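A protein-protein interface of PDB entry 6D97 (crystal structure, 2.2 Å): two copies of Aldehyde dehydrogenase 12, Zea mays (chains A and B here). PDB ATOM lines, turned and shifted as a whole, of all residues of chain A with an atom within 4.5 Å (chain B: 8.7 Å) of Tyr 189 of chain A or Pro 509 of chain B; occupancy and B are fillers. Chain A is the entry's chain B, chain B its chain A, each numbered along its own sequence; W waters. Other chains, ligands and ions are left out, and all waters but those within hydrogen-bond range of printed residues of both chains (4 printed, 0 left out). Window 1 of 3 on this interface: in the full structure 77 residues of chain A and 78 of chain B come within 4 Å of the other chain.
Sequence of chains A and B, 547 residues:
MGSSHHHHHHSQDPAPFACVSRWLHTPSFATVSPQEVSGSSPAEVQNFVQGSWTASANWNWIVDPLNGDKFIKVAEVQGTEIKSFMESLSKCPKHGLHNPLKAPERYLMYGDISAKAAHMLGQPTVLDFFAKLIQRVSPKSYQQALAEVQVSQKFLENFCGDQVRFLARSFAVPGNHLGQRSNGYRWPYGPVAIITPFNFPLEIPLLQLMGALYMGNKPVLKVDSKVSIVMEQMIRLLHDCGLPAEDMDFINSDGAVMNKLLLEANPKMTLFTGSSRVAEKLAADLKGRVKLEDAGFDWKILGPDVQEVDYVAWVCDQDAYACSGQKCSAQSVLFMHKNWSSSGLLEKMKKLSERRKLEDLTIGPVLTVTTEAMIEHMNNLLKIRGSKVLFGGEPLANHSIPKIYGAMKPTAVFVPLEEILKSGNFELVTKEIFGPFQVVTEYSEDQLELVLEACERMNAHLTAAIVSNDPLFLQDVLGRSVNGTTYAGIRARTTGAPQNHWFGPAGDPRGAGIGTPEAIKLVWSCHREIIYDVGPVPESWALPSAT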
ATOM      1  N   LYS A  94     -13.355 -16.924   9.548  1.00  0.00           N
ATOM      2  CA  LYS A  94     -14.680 -17.402   9.916  1.00  0.00           C
ATOM      3  C   LYS A  94     -14.788 -17.732  11.400  1.00  0.00           C
ATOM      4  O   LYS A  94     -15.906 -17.815  11.917  1.00  0.00           O
ATOM      5  CB  LYS A  94     -15.058 -18.615   9.065  1.00  0.00           C
ATOM      6  CG  LYS A  94     -15.409 -18.249   7.636  1.00  0.00           C
ATOM      7  CD  LYS A  94     -15.692 -19.478   6.797  1.00  0.00           C
ATOM      8  CE  LYS A  94     -14.405 -20.208   6.462  1.00  0.00           C
ATOM      9  NZ  LYS A  94     -14.561 -21.156   5.320  1.00  0.00           N
ATOM     10  N   TRP A 187     -20.856 -19.146  18.361  1.00  0.00           N
ATOM     11  CA  TRP A 187     -19.710 -18.843  17.515  1.00  0.00           C
ATOM     12  C   TRP A 187     -20.015 -17.671  16.593  1.00  0.00           C
ATOM     13  O   TRP A 187     -21.141 -17.551  16.100  1.00  0.00           O
ATOM     14  CB  TRP A 187     -19.334 -20.058  16.668  1.00  0.00           C
ATOM     15  CG  TRP A 187     -17.866 -20.337  16.622  1.00  0.00           C
ATOM     16  CD1 TRP A 187     -17.054 -20.274  15.531  1.00  0.00           C
ATOM     17  CD2 TRP A 187     -17.034 -20.728  17.722  1.00  0.00           C
ATOM     18  NE1 TRP A 187     -15.767 -20.604  15.878  1.00  0.00           N
ATOM     19  CE2 TRP A 187     -15.728 -20.886  17.218  1.00  0.00           C
ATOM     20  CE3 TRP A 187     -17.267 -20.963  19.078  1.00  0.00           C
ATOM     21  CZ2 TRP A 187     -14.657 -21.268  18.024  1.00  0.00           C
ATOM     22  CZ3 TRP A 187     -16.205 -21.339  19.878  1.00  0.00           C
ATOM     23  CH2 TRP A 187     -14.917 -21.493  19.349  1.00  0.00           C
ATOM     24  N   PRO A 188     -19.043 -16.804  16.320  1.00  0.00           N
ATOM     25  CA  PRO A 188     -19.278 -15.706  15.379  1.00  0.00           C
ATOM     26  C   PRO A 188     -19.400 -16.231  13.960  1.00  0.00           C
ATOM     27  O   PRO A 188     -19.139 -17.400  13.668  1.00  0.00           O
ATOM     28  CB  PRO A 188     -18.033 -14.832  15.542  1.00  0.00           C
ATOM     29  CG  PRO A 188     -16.959 -15.814  15.878  1.00  0.00           C
ATOM     30  CD  PRO A 188     -17.627 -16.872  16.733  1.00  0.00           C
ATOM     31  N   TYR A 189     -19.812 -15.340  13.061  1.00  0.00           N
ATOM     32  CA  TYR A 189     -19.743 -15.633  11.638  1.00  0.00           C
ATOM     33  C   TYR A 189     -18.480 -15.094  10.986  1.00  0.00           C
ATOM     34  O   TYR A 189     -18.081 -15.603   9.933  1.00  0.00           O
ATOM     35  CB  TYR A 189     -20.961 -15.061  10.904  1.00  0.00           C
ATOM     36  CG  TYR A 189     -22.279 -15.699  11.276  1.00  0.00           C
ATOM     37  CD1 TYR A 189     -22.683 -16.897  10.700  1.00  0.00           C
ATOM     38  CD2 TYR A 189     -23.130 -15.090  12.188  1.00  0.00           C
ATOM     39  CE1 TYR A 189     -23.896 -17.476  11.031  1.00  0.00           C
ATOM     40  CE2 TYR A 189     -24.343 -15.658  12.521  1.00  0.00           C
ATOM     41  CZ  TYR A 189     -24.720 -16.850  11.942  1.00  0.00           C
ATOM     42  OH  TYR A 189     -25.928 -17.415  12.275  1.00  0.00           O
ATOM     43  N   GLY A 190     -17.836 -14.099  11.591  1.00  0.00           N
ATOM     44  CA  GLY A 190     -16.674 -13.481  11.005  1.00  0.00           C
ATOM     45  C   GLY A 190     -17.036 -12.230  10.227  1.00  0.00           C
ATOM     46  O   GLY A 190     -17.583 -11.268  10.772  1.00  0.00           O
ATOM     47  N   PRO A 191     -16.738 -12.229   8.927  1.00  0.00           N
ATOM     48  CA  PRO A 191     -17.037 -11.059   8.080  1.00  0.00           C
ATOM     49  C   PRO A 191     -18.531 -10.956   7.813  1.00  0.00           C
ATOM     50  O   PRO A 191     -19.148 -11.901   7.315  1.00  0.00           O
ATOM     51  CB  PRO A 191     -16.244 -11.341   6.799  1.00  0.00           C
ATOM     52  CG  PRO A 191     -16.160 -12.842   6.744  1.00  0.00           C
ATOM     53  CD  PRO A 191     -16.104 -13.324   8.172  1.00  0.00           C
ATOM     54  N   VAL A 192     -19.120  -9.808   8.160  1.00  0.00           N
ATOM     55  CA  VAL A 192     -20.562  -9.603   8.067  1.00  0.00           C
ATOM     56  C   VAL A 192     -20.847  -8.197   7.548  1.00  0.00           C
ATOM     57  O   VAL A 192     -19.972  -7.330   7.513  1.00  0.00           O
ATOM     58  CB  VAL A 192     -21.276  -9.826   9.417  1.00  0.00           C
ATOM     59  CG1 VAL A 192     -21.041 -11.242   9.930  1.00  0.00           C
ATOM     60  CG2 VAL A 192     -20.810  -8.805  10.438  1.00  0.00           C
ATOM     61  N   ASN A 217     -17.699 -10.692  15.394  1.00  0.00           N
ATOM     62  CA  ASN A 217     -17.709 -10.491  13.954  1.00  0.00           C
ATOM     63  C   ASN A 217     -16.948  -9.219  13.582  1.00  0.00           C
ATOM     64  O   ASN A 217     -16.642  -8.374  14.424  1.00  0.00           O
ATOM     65  CB  ASN A 217     -19.146 -10.412  13.432  1.00  0.00           C
ATOM     66  CG  ASN A 217     -19.972 -11.642  13.778  1.00  0.00           C
ATOM     67  OD1 ASN A 217     -19.854 -12.688  13.134  1.00  0.00           O
ATOM     68  ND2 ASN A 217     -20.831 -11.514  14.786  1.00  0.00           N
ATOM     69  N   LYS A 268     -20.473 -13.732   5.577  1.00  0.00           N
ATOM     70  CA  LYS A 268     -21.121 -14.917   6.125  1.00  0.00           C
ATOM     71  C   LYS A 268     -22.477 -14.606   6.733  1.00  0.00           C
ATOM     72  O   LYS A 268     -23.287 -15.521   6.912  1.00  0.00           O
ATOM     73  CB  LYS A 268     -20.214 -15.580   7.163  1.00  0.00           C
ATOM     74  CG  LYS A 268     -18.901 -16.060   6.572  1.00  0.00           C
ATOM     75  CD  LYS A 268     -19.145 -17.062   5.450  1.00  0.00           C
ATOM     76  CE  LYS A 268     -18.085 -16.960   4.355  1.00  0.00           C
ATOM     77  NZ  LYS A 268     -18.180 -18.086   3.377  1.00  0.00           N
ATOM     78  N   MET A 269     -22.742 -13.342   7.046  1.00  0.00           N
ATOM     79  CA  MET A 269     -24.055 -12.919   7.505  1.00  0.00           C
ATOM     80  C   MET A 269     -24.266 -11.479   7.075  1.00  0.00           C
ATOM     81  O   MET A 269     -23.318 -10.693   6.998  1.00  0.00           O
ATOM     82  CB  MET A 269     -24.201 -13.052   9.025  1.00  0.00           C
ATOM     83  CG  MET A 269     -25.377 -13.912   9.448  1.00  0.00           C
ATOM     84  SD  MET A 269     -26.963 -13.186   9.006  1.00  0.00           S
ATOM     85  CE  MET A 269     -26.900 -11.665   9.949  1.00  0.00           C
ATOM     86  N   GLY A 288     -30.108 -16.603   1.146  1.00  0.00           N
ATOM     87  CA  GLY A 288     -30.624 -16.726   2.488  1.00  0.00           C
ATOM     88  C   GLY A 288     -29.630 -16.537   3.610  1.00  0.00           C
ATOM     89  O   GLY A 288     -30.008 -16.699   4.777  1.00  0.00           O
ATOM     90  N   ARG A 289     -28.377 -16.203   3.312  1.00  0.00           N
ATOM     91  CA  ARG A 289     -27.410 -15.858   4.354  1.00  0.00           C
ATOM     92  C   ARG A 289     -27.664 -14.435   4.858  1.00  0.00           C
ATOM     93  O   ARG A 289     -26.804 -13.555   4.802  1.00  0.00           O
ATOM     94  CB  ARG A 289     -25.988 -16.018   3.829  1.00  0.00           C
ATOM     95  CG  ARG A 289     -25.508 -17.461   3.760  1.00  0.00           C
ATOM     96  CD  ARG A 289     -24.083 -17.543   3.251  1.00  0.00           C
ATOM     97  NE  ARG A 289     -23.484 -18.846   3.527  1.00  0.00           N
ATOM     98  CZ  ARG A 289     -22.896 -19.160   4.673  1.00  0.00           C
ATOM     99  NH1 ARG A 289     -22.842 -18.262   5.647  1.00  0.00           N
ATOM    100  NH2 ARG A 289     -22.368 -20.365   4.847  1.00  0.00           N
ATOM    101  N   VAL A 290     -28.888 -14.220   5.352  1.00  0.00           N
ATOM    102  CA  VAL A 290     -29.350 -12.899   5.772  1.00  0.00           C
ATOM    103  C   VAL A 290     -30.212 -13.025   7.028  1.00  0.00           C
ATOM    104  O   VAL A 290     -30.753 -14.096   7.330  1.00  0.00           O
ATOM    105  CB  VAL A 290     -30.160 -12.182   4.664  1.00  0.00           C
ATOM    106  CG1 VAL A 290     -29.328 -11.990   3.395  1.00  0.00           C
ATOM    107  CG2 VAL A 290     -31.431 -12.967   4.327  1.00  0.00           C
ATOM    108  N   LYS A 291     -30.328 -11.904   7.756  1.00  0.00           N
ATOM    109  CA  LYS A 291     -31.369 -11.665   8.738  1.00  0.00           C
ATOM    110  C   LYS A 291     -32.062 -10.367   8.344  1.00  0.00           C
ATOM    111  O   LYS A 291     -31.402  -9.404   7.916  1.00  0.00           O
ATOM    112  CB  LYS A 291     -30.810 -11.563  10.172  1.00  0.00           C
ATOM    113  CG  LYS A 291     -30.176 -12.858  10.663  1.00  0.00           C
ATOM    114  CD  LYS A 291     -31.228 -13.940  10.845  1.00  0.00           C
ATOM    115  CE  LYS A 291     -30.637 -15.216  11.435  1.00  0.00           C
ATOM    116  NZ  LYS A 291     -31.660 -16.277  11.611  1.00  0.00           N
ATOM    117  N   VAL A 523     -28.971 -13.109  15.932  1.00  0.00           N
ATOM    118  CA  VAL A 523     -28.602 -12.480  14.674  1.00  0.00           C
ATOM    119  C   VAL A 523     -27.112 -12.618  14.389  1.00  0.00           C
ATOM    120  O   VAL A 523     -26.716 -12.801  13.233  1.00  0.00           O
ATOM    121  CB  VAL A 523     -29.036 -11.003  14.691  1.00  0.00           C
ATOM    122  CG1 VAL A 523     -28.467 -10.273  13.496  1.00  0.00           C
ATOM    123  CG2 VAL A 523     -30.549 -10.904  14.698  1.00  0.00           C
ATOM    124  N   TRP A 524     -26.261 -12.554  15.415  1.00  0.00           N
ATOM    125  CA  TRP A 524     -24.833 -12.353  15.201  1.00  0.00           C
ATOM    126  C   TRP A 524     -23.965 -13.525  15.637  1.00  0.00           C
ATOM    127  O   TRP A 524     -22.734 -13.399  15.645  1.00  0.00           O
ATOM    128  CB  TRP A 524     -24.381 -11.073  15.903  1.00  0.00           C
ATOM    129  CG  TRP A 524     -24.989  -9.871  15.281  1.00  0.00           C
ATOM    130  CD1 TRP A 524     -25.803  -8.950  15.878  1.00  0.00           C
ATOM    131  CD2 TRP A 524     -24.858  -9.470  13.917  1.00  0.00           C
ATOM    132  NE1 TRP A 524     -26.174  -7.992  14.966  1.00  0.00           N
ATOM    133  CE2 TRP A 524     -25.604  -8.286  13.757  1.00  0.00           C
ATOM    134  CE3 TRP A 524     -24.170  -9.991  12.817  1.00  0.00           C
ATOM    135  CZ2 TRP A 524     -25.691  -7.623  12.536  1.00  0.00           C
ATOM    136  CZ3 TRP A 524     -24.254  -9.332  11.612  1.00  0.00           C
ATOM    137  CH2 TRP A 524     -25.009  -8.160  11.479  1.00  0.00           C
ATOM    138  N   SER A 525     -24.560 -14.660  15.991  1.00  0.00           N
ATOM    139  CA  SER A 525     -23.792 -15.856  16.285  1.00  0.00           C
ATOM    140  C   SER A 525     -24.560 -17.069  15.784  1.00  0.00           C
ATOM    141  O   SER A 525     -25.748 -16.996  15.459  1.00  0.00           O
ATOM    142  CB  SER A 525     -23.487 -15.989  17.784  1.00  0.00           C
ATOM    143  OG  SER A 525     -24.651 -16.315  18.522  1.00  0.00           O
ATOM    144  N   CYS A 526     -23.850 -18.189  15.703  1.00  0.00           N
ATOM    145  CA  CYS A 526     -24.438 -19.483  15.405  1.00  0.00           C
ATOM    146  C   CYS A 526     -23.998 -20.460  16.482  1.00  0.00           C
ATOM    147  O   CYS A 526     -23.086 -20.186  17.266  1.00  0.00           O
ATOM    148  CB  CYS A 526     -24.030 -19.988  14.015  1.00  0.00           C
ATOM    149  SG  CYS A 526     -22.255 -20.114  13.750  1.00  0.00           S
ATOM    150  N   MET B 269     -41.470 -22.632   6.416  1.00  0.00           N
ATOM    151  CA  MET B 269     -40.133 -23.108   6.736  1.00  0.00           C
ATOM    152  C   MET B 269     -39.909 -24.416   5.995  1.00  0.00           C
ATOM    153  O   MET B 269     -40.829 -25.223   5.864  1.00  0.00           O
ATOM    154  CB  MET B 269     -39.946 -23.311   8.245  1.00  0.00           C
ATOM    155  CG  MET B 269     -38.742 -22.573   8.826  1.00  0.00           C
ATOM    156  SD  MET B 269     -37.165 -23.123   8.139  1.00  0.00           S
ATOM    157  CE  MET B 269     -37.140 -24.829   8.681  1.00  0.00           C
ATOM    158  N   GLY B 288     -34.207 -18.091   1.093  1.00  0.00           N
ATOM    159  CA  GLY B 288     -33.649 -18.239   2.417  1.00  0.00           C
ATOM    160  C   GLY B 288     -34.608 -18.698   3.489  1.00  0.00           C
ATOM    161  O   GLY B 288     -34.212 -18.767   4.659  1.00  0.00           O
ATOM    162  N   VAL B 290     -35.336 -21.359   4.733  1.00  0.00           N
ATOM    163  CA  VAL B 290     -34.872 -22.735   4.854  1.00  0.00           C
ATOM    164  C   VAL B 290     -33.984 -22.875   6.080  1.00  0.00           C
ATOM    165  O   VAL B 290     -33.427 -21.901   6.590  1.00  0.00           O
ATOM    166  CB  VAL B 290     -34.082 -23.198   3.605  1.00  0.00           C
ATOM    167  CG1 VAL B 290     -34.978 -23.270   2.395  1.00  0.00           C
ATOM    168  CG2 VAL B 290     -32.905 -22.263   3.342  1.00  0.00           C
ATOM    169  N   LYS B 291     -33.855 -24.111   6.548  1.00  0.00           N
ATOM    170  CA  LYS B 291     -32.757 -24.532   7.402  1.00  0.00           C
ATOM    171  C   LYS B 291     -32.058 -25.690   6.707  1.00  0.00           C
ATOM    172  O   LYS B 291     -32.713 -26.584   6.160  1.00  0.00           O
ATOM    173  CB  LYS B 291     -33.230 -24.951   8.799  1.00  0.00           C
ATOM    174  CG  LYS B 291     -33.738 -23.811   9.665  1.00  0.00           C
ATOM    175  CD  LYS B 291     -32.643 -22.815  10.012  1.00  0.00           C
ATOM    176  CE  LYS B 291     -33.194 -21.695  10.889  1.00  0.00           C
ATOM    177  NZ  LYS B 291     -32.244 -20.556  10.996  1.00  0.00           N
ATOM    178  N   LEU B 292     -30.731 -25.662   6.707  1.00  0.00           N
ATOM    179  CA  LEU B 292     -29.945 -26.572   5.893  1.00  0.00           C
ATOM    180  C   LEU B 292     -29.071 -27.458   6.766  1.00  0.00           C
ATOM    181  O   LEU B 292     -28.419 -26.982   7.701  1.00  0.00           O
ATOM    182  CB  LEU B 292     -29.066 -25.802   4.902  1.00  0.00           C
ATOM    183  CG  LEU B 292     -29.813 -24.897   3.922  1.00  0.00           C
ATOM    184  CD1 LEU B 292     -28.843 -24.128   3.038  1.00  0.00           C
ATOM    185  CD2 LEU B 292     -30.771 -25.723   3.077  1.00  0.00           C
ATOM    186  N   GLU B 456      -9.699 -23.574   7.154  1.00  0.00           N
ATOM    187  CA  GLU B 456     -10.414 -22.318   6.953  1.00  0.00           C
ATOM    188  C   GLU B 456     -10.814 -22.126   5.494  1.00  0.00           C
ATOM    189  O   GLU B 456     -11.837 -21.494   5.210  1.00  0.00           O
ATOM    190  CB  GLU B 456      -9.553 -21.152   7.443  1.00  0.00           C
ATOM    191  CG  GLU B 456     -10.088 -19.766   7.118  1.00  0.00           C
ATOM    192  CD  GLU B 456     -11.241 -19.344   8.011  1.00  0.00           C
ATOM    193  OE1 GLU B 456     -11.599 -20.109   8.935  1.00  0.00           O
ATOM    194  OE2 GLU B 456     -11.787 -18.240   7.787  1.00  0.00           O
ATOM    195  N   HIS B 461     -18.464 -26.811   7.061  1.00  0.00           N
ATOM    196  CA  HIS B 461     -18.025 -26.850   8.453  1.00  0.00           C
ATOM    197  C   HIS B 461     -19.044 -27.663   9.257  1.00  0.00           C
ATOM    198  O   HIS B 461     -19.801 -27.128  10.068  1.00  0.00           O
ATOM    199  CB  HIS B 461     -17.848 -25.437   9.006  1.00  0.00           C
ATOM    200  CG  HIS B 461     -16.892 -24.599   8.216  1.00  0.00           C
ATOM    201  ND1 HIS B 461     -15.554 -24.907   8.104  1.00  0.00           N
ATOM    202  CD2 HIS B 461     -17.081 -23.476   7.486  1.00  0.00           C
ATOM    203  CE1 HIS B 461     -14.958 -24.005   7.345  1.00  0.00           C
ATOM    204  NE2 HIS B 461     -15.863 -23.124   6.959  1.00  0.00           N
ATOM    205  N   VAL B 482     -14.146 -23.792  12.935  1.00  0.00           N
ATOM    206  CA  VAL B 482     -15.553 -23.402  12.854  1.00  0.00           C
ATOM    207  C   VAL B 482     -16.510 -24.575  13.072  1.00  0.00           C
ATOM    208  O   VAL B 482     -17.575 -24.401  13.678  1.00  0.00           O
ATOM    209  CB  VAL B 482     -15.838 -22.721  11.498  1.00  0.00           C
ATOM    210  CG1 VAL B 482     -17.330 -22.489  11.298  1.00  0.00           C
ATOM    211  CG2 VAL B 482     -15.084 -21.404  11.385  1.00  0.00           C
ATOM    212  N   TRP B 502     -26.011 -31.566  20.181  1.00  0.00           N
ATOM    213  CA  TRP B 502     -26.263 -30.978  18.876  1.00  0.00           C
ATOM    214  C   TRP B 502     -25.494 -31.696  17.774  1.00  0.00           C
ATOM    215  O   TRP B 502     -24.348 -32.115  17.960  1.00  0.00           O
ATOM    216  CB  TRP B 502     -25.868 -29.499  18.931  1.00  0.00           C
ATOM    217  CG  TRP B 502     -25.715 -28.800  17.616  1.00  0.00           C
ATOM    218  CD1 TRP B 502     -24.672 -28.907  16.732  1.00  0.00           C
ATOM    219  CD2 TRP B 502     -26.614 -27.837  17.058  1.00  0.00           C
ATOM    220  NE1 TRP B 502     -24.885 -28.090  15.649  1.00  0.00           N
ATOM    221  CE2 TRP B 502     -26.066 -27.419  15.826  1.00  0.00           C
ATOM    222  CE3 TRP B 502     -27.833 -27.289  17.476  1.00  0.00           C
ATOM    223  CZ2 TRP B 502     -26.700 -26.486  15.004  1.00  0.00           C
ATOM    224  CZ3 TRP B 502     -28.460 -26.362  16.659  1.00  0.00           C
ATOM    225  CH2 TRP B 502     -27.887 -25.968  15.438  1.00  0.00           C
ATOM    226  N   PRO B 505     -24.116 -28.032  11.191  1.00  0.00           N
ATOM    227  CA  PRO B 505     -22.972 -27.210  10.793  1.00  0.00           C
ATOM    228  C   PRO B 505     -22.929 -25.920  11.608  1.00  0.00           C
ATOM    229  O   PRO B 505     -23.817 -25.626  12.404  1.00  0.00           O
ATOM    230  CB  PRO B 505     -23.245 -26.940   9.314  1.00  0.00           C
ATOM    231  CG  PRO B 505     -24.736 -26.913   9.230  1.00  0.00           C
ATOM    232  CD  PRO B 505     -25.221 -27.942  10.219  1.00  0.00           C
ATOM    233  N   ALA B 506     -21.859 -25.155  11.400  1.00  0.00           N
ATOM    234  CA  ALA B 506     -21.731 -23.806  11.934  1.00  0.00           C
ATOM    235  C   ALA B 506     -21.285 -22.869  10.820  1.00  0.00           C
ATOM    236  O   ALA B 506     -20.924 -23.297   9.721  1.00  0.00           O
ATOM    237  CB  ALA B 506     -20.740 -23.739  13.102  1.00  0.00           C
ATOM    238  N   GLY B 507     -21.301 -21.572  11.124  1.00  0.00           N
ATOM    239  CA  GLY B 507     -20.882 -20.573  10.160  1.00  0.00           C
ATOM    240  C   GLY B 507     -21.922 -20.205   9.130  1.00  0.00           C
ATOM    241  O   GLY B 507     -21.572 -19.652   8.083  1.00  0.00           O
ATOM    242  N   ASP B 508     -23.195 -20.477   9.401  1.00  0.00           N
ATOM    243  CA  ASP B 508     -24.267 -20.245   8.443  1.00  0.00           C
ATOM    244  C   ASP B 508     -25.559 -19.938   9.192  1.00  0.00           C
ATOM    245  O   ASP B 508     -26.013 -20.757  10.001  1.00  0.00           O
ATOM    246  CB  ASP B 508     -24.428 -21.473   7.537  1.00  0.00           C
ATOM    247  CG  ASP B 508     -25.469 -21.283   6.442  1.00  0.00           C
ATOM    248  OD1 ASP B 508     -26.115 -20.215   6.380  1.00  0.00           O
ATOM    249  OD2 ASP B 508     -25.635 -22.221   5.633  1.00  0.00           O
ATOM    250  N   PRO B 509     -26.176 -18.773   8.962  1.00  0.00           N
ATOM    251  CA  PRO B 509     -27.470 -18.494   9.613  1.00  0.00           C
ATOM    252  C   PRO B 509     -28.560 -19.462   9.210  1.00  0.00           C
ATOM    253  O   PRO B 509     -29.592 -19.534   9.889  1.00  0.00           O
ATOM    254  CB  PRO B 509     -27.800 -17.067   9.152  1.00  0.00           C
ATOM    255  CG  PRO B 509     -27.018 -16.882   7.897  1.00  0.00           C
ATOM    256  CD  PRO B 509     -25.751 -17.672   8.080  1.00  0.00           C
ATOM    257  N   ARG B 510     -28.374 -20.191   8.116  1.00  0.00           N
ATOM    258  CA  ARG B 510     -29.315 -21.213   7.696  1.00  0.00           C
ATOM    259  C   ARG B 510     -29.021 -22.567   8.321  1.00  0.00           C
ATOM    260  O   ARG B 510     -29.792 -23.509   8.110  1.00  0.00           O
ATOM    261  CB  ARG B 510     -29.295 -21.345   6.171  1.00  0.00           C
ATOM    262  CG  ARG B 510     -29.452 -20.027   5.433  1.00  0.00           C
ATOM    263  CD  ARG B 510     -28.971 -20.156   4.001  1.00  0.00           C
ATOM    264  NE  ARG B 510     -27.640 -20.754   3.927  1.00  0.00           N
ATOM    265  CZ  ARG B 510     -27.000 -21.020   2.792  1.00  0.00           C
ATOM    266  NH1 ARG B 510     -27.567 -20.740   1.628  1.00  0.00           N
ATOM    267  NH2 ARG B 510     -25.794 -21.570   2.822  1.00  0.00           N
ATOM    268  N   GLY B 511     -27.930 -22.683   9.076  1.00  0.00           N
ATOM    269  CA  GLY B 511     -27.525 -23.946   9.662  1.00  0.00           C
ATOM    270  C   GLY B 511     -28.577 -24.576  10.546  1.00  0.00           C
ATOM    271  O   GLY B 511     -29.053 -23.959  11.504  1.00  0.00           O
ATOM    272  N   ALA B 512     -28.958 -25.802  10.220  1.00  0.00           N
ATOM    273  CA  ALA B 512     -29.912 -26.547  11.020  1.00  0.00           C
ATOM    274  C   ALA B 512     -29.191 -27.385  12.068  1.00  0.00           C
ATOM    275  O   ALA B 512     -28.017 -27.736  11.927  1.00  0.00           O
ATOM    276  CB  ALA B 512     -30.773 -27.446  10.132  1.00  0.00           C
ATOM    277  N   LEU B 522     -34.743 -23.971  17.573  1.00  0.00           N
ATOM    278  CA  LEU B 522     -34.138 -23.115  16.554  1.00  0.00           C
ATOM    279  C   LEU B 522     -34.739 -23.383  15.180  1.00  0.00           C
ATOM    280  O   LEU B 522     -35.064 -22.448  14.438  1.00  0.00           O
ATOM    281  CB  LEU B 522     -32.624 -23.329  16.522  1.00  0.00           C
ATOM    282  CG  LEU B 522     -31.928 -22.861  15.242  1.00  0.00           C
ATOM    283  CD1 LEU B 522     -31.761 -21.345  15.266  1.00  0.00           C
ATOM    284  CD2 LEU B 522     -30.594 -23.561  15.044  1.00  0.00           C
ATOM    285  N   VAL B 523     -34.910 -24.655  14.833  1.00  0.00           N
ATOM    286  CA  VAL B 523     -35.295 -25.011  13.473  1.00  0.00           C
ATOM    287  C   VAL B 523     -36.790 -24.820  13.250  1.00  0.00           C
ATOM    288  O   VAL B 523     -37.214 -24.391  12.171  1.00  0.00           O
ATOM    289  CB  VAL B 523     -34.852 -26.457  13.174  1.00  0.00           C
ATOM    290  CG1 VAL B 523     -35.451 -26.943  11.874  1.00  0.00           C
ATOM    291  CG2 VAL B 523     -33.335 -26.538  13.111  1.00  0.00           C
HETATM  292  O   HOH W   1     -18.621 -18.341   9.412  1.00  0.00           O
HETATM  293  O   HOH W   2     -33.872 -18.675  12.357  1.00  0.00           O
HETATM  294  O   HOH W   3     -27.410 -20.251  12.533  1.00  0.00           O
HETATM  295  O   HOH W   4     -32.070 -17.841   6.389  1.00  0.00           O
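Gly 288 of chain B touches its own counterpart, Gly 288 of chain A.
Positions printed for both chains: 269, 288, 290, 291 and 523.
Of the 16 pairs that touch across the chains among the printed residues, 1 has its exchanged pair printed and touching as well.
Water W1 lies within hydrogen-bond range of O of Tyr 189 of chain A (2.8 Å) and O of Gly 507 of chain B (3.5 Å).
Water W4 bridges O of Gly 288 of chain A (2.9 Å) and O of Gly 288 of chain B (2.9 Å).
Water W3 lies within hydrogen-bond range of the backbone carbonyl oxygen (O) of Asp 508 of chain B and the side-chain hydroxyl (OH) of Tyr 189 of chain A.
Of the 18 printed residues of chain A, 7 touch a printed residue of chain B.
Hydrophobic or aromatic side chains of chain A that line the printed part of chain B: Tyr 189 and Met 269.
Of the 19 printed residues of chain B, 9 touch a printed residue of chain A.
Among the printed residues, 16 pairs touch across the chains.
Among the printed residues, Asp or Glu carboxylates within 4 Å of a Lys or Arg side-chain nitrogen of the other chain: Arg 289 of chain A with Asp 508 of chain B.
The side-chain carboxylate (OD2) of Asp 508 of chain B is in salt-bridge range of the guanidinium group (NH2) of Arg 289 of chain A, 3.8 Å away.
The side-chain carboxylate (OE2) of Glu 456 of chain B lies within hydrogen-bond range of the backbone NH (N) of Lys 94 of chain A.
O of Gly 507 of chain B sits at hydrogen-bond distance from NH1 of Arg 289 of chain A, 3.1 Å away.
N of Gly 507 of chain B lies within hydrogen-bond range of SG of Cys 526 of chain A.
NZ of Lys 94 of chain A is in hydrogen-bond range of NE2 of His 461 of chain B, 2.9 Å away.
NH2 of Arg 510 of chain B is in salt-bridge range of OD2 of Asp 508 of chain B, 2.9 Å away.
The backbone carbonyl oxygen of Lys 268 of chain A lies within hydrogen-bond range of the guanidinium group of Arg 289 of chain A, 3.1 Å away.
N of Tyr 189 of chain A lies within hydrogen-bond range of OD1 of Asn 217 of chain A (2.7 Å).
No residue of chain B comes within 4 Å of Pro 188 of chain A.
Of chain B, only Gly 507 (3.7 Å), Asp 508 (3.5 Å) and Pro 509 (3.3 Å) come within 4 Å of Tyr 189 of chain A.
No residue of chain B comes within 4 Å of Gly 190 of chain A.
Lys 291 of chain B touches none of the printed residues of chain A.
Printed residues of chain A within 4 Å of Glu 456 of chain B: Lys 94.
Of the printed residues of chain A, His 461 of chain B touches Lys 94 (2.9 Å).
Pro 509 of chain B touches just these residues of chain A: Tyr 189, Lys 268, Met 269 and Arg 289.
Gly 511 of chain B touches none of the printed residues of chain A.
The nearest residue of chain B that does not touch Tyr 189 of chain A is Arg 510 of chain B (5.6 Å).
CG2 of Val 482 of chain B touches CB of Lys 94 of chain A (3.6 Å).
Asp 508 of chain B touches Tyr 189 of chain A (N to CE1, 3.5 Å).
Tyr 189 of chain A touches Pro 509 of chain B (OH to CA, 3.3 Å).
Lys 268 of chain A touches Pro 509 of chain B.
Arg 289 of chain A touches Pro 509 of chain B.
Arg 289 of chain A touches Arg 510 of chain B.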
